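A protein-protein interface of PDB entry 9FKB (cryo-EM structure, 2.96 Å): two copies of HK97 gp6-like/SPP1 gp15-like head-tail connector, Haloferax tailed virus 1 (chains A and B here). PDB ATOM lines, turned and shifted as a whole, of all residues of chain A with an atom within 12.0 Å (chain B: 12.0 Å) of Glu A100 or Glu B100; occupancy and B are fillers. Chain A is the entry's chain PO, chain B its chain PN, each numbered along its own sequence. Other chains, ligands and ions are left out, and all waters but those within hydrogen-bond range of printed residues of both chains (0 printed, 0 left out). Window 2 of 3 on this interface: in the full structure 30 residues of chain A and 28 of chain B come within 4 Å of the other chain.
Of chain B, only Glu B100 (3.9 Å) comes within 4 Å of Glu A100. Of chain A, only Glu A100 (3.9 Å) comes within 4 Å of Glu B100. Of chain B, only Gly B102 (3.4 Å) and Ser B103 (2.8 Å) come within 4 Å of Ser A98. No residue of chain B comes within 4 Å of Gly A99. No residue of chain B comes within 4 Å of Gly A101. No residue of chain B comes within 4 Å of Gly A102. No residue of chain A comes within 4 Å of Ser B98. No residue of chain A comes within 4 Å of Gly B99. No residue of chain A comes within 4 Å of Gly B101. Printed residues of chain A within 4 Å of Ser B103: Glu A97 and Ser A98. Printed residues of chain B within 4 Å of Glu A97: Ser B103 (3.6 Å). Printed residues of chain B within 4 Å of Ser A96: Val B104. Printed residues of chain A within 4 Å of Val B104: Ser A96 (3.3 Å). Val A104 touches none of the printed residues of chain B. Ser A103 touches none of the printed residues of chain B. The nearest residue of chain A that does not touch Glu B100 is Gly A99 (7.0 Å). The nearest printed residue of chain B that does not touch Glu A97 is Val B104 (4.2 Å).
Among the printed residues, pairs that only touch across the chains: Ser A96 with Val B104 (3.3 Å), Glu A97 with Ser B103 (3.6 Å), Ser A98 with Gly B102 (3.4 Å) and Glu A100 with Glu B100 (3.9 Å).
OG of Ser B96 sits at hydrogen-bond distance from O of Val B104 (3.4 Å). The backbone carbonyl oxygen of Glu B97 sits at hydrogen-bond distance from the backbone NH of Val B104, 2.9 Å away. OG of Ser B98 is in hydrogen-bond range of OG of Ser B103, 2.7 Å away. OG of Ser A96 sits close to O of Val A104 (3.5 Å). The backbone NH (N) of Glu A97 sits at hydrogen-bond distance from the backbone carbonyl oxygen (O) of Val A104 (2.9 Å). The side-chain hydroxyl of Ser A103 is in hydrogen-bond range of the side-chain hydroxyl of Ser A98 (2.7 Å).
O of Ser B103 sits at hydrogen-bond distance from N of Ser A98, at 2.8 Å.
Ser A96 touches Val B104, but with the chains exchanged Val A104 does not touch Ser B96 (11.3 Å). Glu A97 touches Ser B103, but with the chains exchanged Ser A103 does not touch Glu B97 (10.8 Å). Ser A98 touches Gly B102, but with the chains exchanged Gly A102 does not touch Ser B98 (11.3 Å). Glu B100 touches its own counterpart, Glu A100. 9 positions are printed for both chains. Of the 5 pairs that touch across the chains among the printed residues, 1 has its exchanged pair printed and touching as well.
Hydrophobic or aromatic side chains of chain B that line the printed part of chain A: Val B104. Among the printed residues, 5 pairs touch across the chains. Among the printed residues, no Asp or Glu carboxylate lies within 4 Å of a Lys or Arg side-chain nitrogen of the other chain.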
ATOM      1  N   SER A  96       2.681 -29.980   7.441  1.00  0.00           N
ATOM      2  CA  SER A  96       1.685 -30.557   8.339  1.00  0.00           C
ATOM      3  C   SER A  96       0.564 -29.542   8.613  1.00  0.00           C
ATOM      4  O   SER A  96       0.814 -28.342   8.694  1.00  0.00           O
ATOM      5  CB  SER A  96       2.346 -31.023   9.608  1.00  0.00           C
ATOM      6  OG  SER A  96       1.408 -31.651  10.465  1.00  0.00           O
ATOM      7  N   GLU A  97      -0.681 -30.032   8.731  1.00  0.00           N
ATOM      8  CA  GLU A  97      -1.823 -29.266   9.214  1.00  0.00           C
ATOM      9  C   GLU A  97      -2.595 -30.092  10.240  1.00  0.00           C
ATOM     10  O   GLU A  97      -2.813 -31.285  10.049  1.00  0.00           O
ATOM     11  CB  GLU A  97      -2.770 -28.873   8.084  1.00  0.00           C
ATOM     12  CG  GLU A  97      -2.265 -27.692   7.262  1.00  0.00           C
ATOM     13  CD  GLU A  97      -3.103 -27.341   6.035  1.00  0.00           C
ATOM     14  OE1 GLU A  97      -3.473 -28.254   5.288  1.00  0.00           O
ATOM     15  OE2 GLU A  97      -3.378 -26.129   5.819  1.00  0.00           O
ATOM     16  N   SER A  98      -3.046 -29.415  11.304  1.00  0.00           N
ATOM     17  CA  SER A  98      -3.667 -30.059  12.452  1.00  0.00           C
ATOM     18  C   SER A  98      -4.764 -29.158  13.032  1.00  0.00           C
ATOM     19  O   SER A  98      -4.479 -28.056  13.497  1.00  0.00           O
ATOM     20  CB  SER A  98      -2.602 -30.391  13.471  1.00  0.00           C
ATOM     21  OG  SER A  98      -3.156 -31.052  14.595  1.00  0.00           O
ATOM     22  N   GLY A  99      -6.022 -29.632  12.985  1.00  0.00           N
ATOM     23  CA  GLY A  99      -7.166 -28.966  13.595  1.00  0.00           C
ATOM     24  C   GLY A  99      -7.395 -29.427  15.035  1.00  0.00           C
ATOM     25  O   GLY A  99      -6.448 -29.577  15.809  1.00  0.00           O
ATOM     26  N   GLU A 100      -8.669 -29.663  15.386  1.00  0.00           N
ATOM     27  CA  GLU A 100      -9.061 -30.232  16.671  1.00  0.00           C
ATOM     28  C   GLU A 100      -8.727 -31.729  16.720  1.00  0.00           C
ATOM     29  O   GLU A 100      -9.609 -32.582  16.594  1.00  0.00           O
ATOM     30  CB  GLU A 100     -10.531 -29.905  16.963  1.00  0.00           C
ATOM     31  CG  GLU A 100     -10.864 -28.419  16.895  1.00  0.00           C
ATOM     32  CD  GLU A 100      -9.989 -27.513  17.745  1.00  0.00           C
ATOM     33  OE1 GLU A 100      -9.869 -27.777  18.964  1.00  0.00           O
ATOM     34  OE2 GLU A 100      -9.435 -26.537  17.189  1.00  0.00           O
ATOM     35  N   GLY A 101      -7.443 -32.047  16.937  1.00  0.00           N
ATOM     36  CA  GLY A 101      -6.966 -33.427  16.958  1.00  0.00           C
ATOM     37  C   GLY A 101      -6.717 -34.008  15.561  1.00  0.00           C
ATOM     38  O   GLY A 101      -5.665 -34.613  15.316  1.00  0.00           O
ATOM     39  N   GLY A 102      -7.675 -33.824  14.635  1.00  0.00           N
ATOM     40  CA  GLY A 102      -7.540 -34.266  13.248  1.00  0.00           C
ATOM     41  C   GLY A 102      -6.312 -33.654  12.571  1.00  0.00           C
ATOM     42  O   GLY A 102      -6.127 -32.444  12.625  1.00  0.00           O
ATOM     43  N   SER A 103      -5.454 -34.497  11.963  1.00  0.00           N
ATOM     44  CA  SER A 103      -4.119 -34.087  11.519  1.00  0.00           C
ATOM     45  C   SER A 103      -3.678 -34.797  10.230  1.00  0.00           C
ATOM     46  O   SER A 103      -4.009 -35.968  10.023  1.00  0.00           O
ATOM     47  CB  SER A 103      -3.095 -34.311  12.607  1.00  0.00           C
ATOM     48  OG  SER A 103      -3.450 -33.651  13.816  1.00  0.00           O
ATOM     49  N   VAL A 104      -2.864 -34.107   9.402  1.00  0.00           N
ATOM     50  CA  VAL A 104      -2.446 -34.577   8.076  1.00  0.00           C
ATOM     51  C   VAL A 104      -1.103 -33.948   7.668  1.00  0.00           C
ATOM     52  O   VAL A 104      -0.804 -32.823   8.059  1.00  0.00           O
ATOM     53  CB  VAL A 104      -3.543 -34.330   7.011  1.00  0.00           C
ATOM     54  CG1 VAL A 104      -3.865 -32.853   6.797  1.00  0.00           C
ATOM     55  CG2 VAL A 104      -3.215 -34.988   5.688  1.00  0.00           C
ATOM     56  N   SER B  96       6.828 -23.000  11.479  1.00  0.00           N
ATOM     57  CA  SER B  96       5.799 -23.689  12.264  1.00  0.00           C
ATOM     58  C   SER B  96       5.015 -22.686  13.121  1.00  0.00           C
ATOM     59  O   SER B  96       5.594 -21.719  13.607  1.00  0.00           O
ATOM     60  CB  SER B  96       6.417 -24.786  13.097  1.00  0.00           C
ATOM     61  OG  SER B  96       5.440 -25.408  13.917  1.00  0.00           O
ATOM     62  N   GLU B  97       3.697 -22.906  13.279  1.00  0.00           N
ATOM     63  CA  GLU B  97       2.821 -22.118  14.145  1.00  0.00           C
ATOM     64  C   GLU B  97       1.818 -23.046  14.843  1.00  0.00           C
ATOM     65  O   GLU B  97       1.365 -24.033  14.274  1.00  0.00           O
ATOM     66  CB  GLU B  97       2.014 -21.071  13.374  1.00  0.00           C
ATOM     67  CG  GLU B  97       2.822 -19.969  12.685  1.00  0.00           C
ATOM     68  CD  GLU B  97       1.908 -19.019  11.901  1.00  0.00           C
ATOM     69  OE1 GLU B  97       1.519 -19.368  10.759  1.00  0.00           O
ATOM     70  OE2 GLU B  97       1.563 -17.924  12.434  1.00  0.00           O
ATOM     71  N   SER B  98       1.436 -22.696  16.078  1.00  0.00           N
ATOM     72  CA  SER B  98       0.595 -23.552  16.915  1.00  0.00           C
ATOM     73  C   SER B  98      -0.169 -22.717  17.954  1.00  0.00           C
ATOM     74  O   SER B  98       0.310 -21.675  18.400  1.00  0.00           O
ATOM     75  CB  SER B  98       1.447 -24.628  17.556  1.00  0.00           C
ATOM     76  OG  SER B  98       0.679 -25.493  18.374  1.00  0.00           O
ATOM     77  N   GLY B  99      -1.361 -23.190  18.355  1.00  0.00           N
ATOM     78  CA  GLY B  99      -2.179 -22.600  19.407  1.00  0.00           C
ATOM     79  C   GLY B  99      -3.521 -23.325  19.531  1.00  0.00           C
ATOM     80  O   GLY B  99      -3.694 -24.405  18.954  1.00  0.00           O
ATOM     81  N   GLU B 100      -4.479 -22.727  20.256  1.00  0.00           N
ATOM     82  CA  GLU B 100      -5.852 -23.223  20.296  1.00  0.00           C
ATOM     83  C   GLU B 100      -6.626 -22.978  18.993  1.00  0.00           C
ATOM     84  O   GLU B 100      -7.785 -23.382  18.878  1.00  0.00           O
ATOM     85  CB  GLU B 100      -6.584 -22.741  21.547  1.00  0.00           C
ATOM     86  CG  GLU B 100      -6.050 -23.383  22.828  1.00  0.00           C
ATOM     87  CD  GLU B 100      -6.096 -24.905  22.892  1.00  0.00           C
ATOM     88  OE1 GLU B 100      -7.109 -25.500  22.433  1.00  0.00           O
ATOM     89  OE2 GLU B 100      -5.152 -25.509  23.473  1.00  0.00           O
ATOM     90  N   GLY B 101      -5.967 -22.348  18.017  1.00  0.00           N
ATOM     91  CA  GLY B 101      -6.399 -22.371  16.624  1.00  0.00           C
ATOM     92  C   GLY B 101      -5.949 -23.618  15.855  1.00  0.00           C
ATOM     93  O   GLY B 101      -6.147 -23.686  14.643  1.00  0.00           O
ATOM     94  N   GLY B 102      -5.339 -24.601  16.535  1.00  0.00           N
ATOM     95  CA  GLY B 102      -4.657 -25.724  15.898  1.00  0.00           C
ATOM     96  C   GLY B 102      -3.265 -25.349  15.380  1.00  0.00           C
ATOM     97  O   GLY B 102      -2.740 -24.282  15.699  1.00  0.00           O
ATOM     98  N   SER B 103      -2.638 -26.260  14.608  1.00  0.00           N
ATOM     99  CA  SER B 103      -1.205 -26.184  14.308  1.00  0.00           C
ATOM    100  C   SER B 103      -0.875 -26.460  12.836  1.00  0.00           C
ATOM    101  O   SER B 103      -1.592 -27.175  12.141  1.00  0.00           O
ATOM    102  CB  SER B 103      -0.393 -27.093  15.202  1.00  0.00           C
ATOM    103  OG  SER B 103      -0.738 -26.935  16.567  1.00  0.00           O
ATOM    104  N   VAL B 104       0.266 -25.917  12.380  1.00  0.00           N
ATOM    105  CA  VAL B 104       0.689 -25.937  10.984  1.00  0.00           C
ATOM    106  C   VAL B 104       2.220 -25.925  10.898  1.00  0.00           C
ATOM    107  O   VAL B 104       2.894 -25.319  11.732  1.00  0.00           O
ATOM    108  CB  VAL B 104       0.056 -24.764  10.196  1.00  0.00           C
ATOM    109  CG1 VAL B 104       0.379 -23.398  10.785  1.00  0.00           C
ATOM    110  CG2 VAL B 104       0.432 -24.753   8.724  1.00  0.00           C
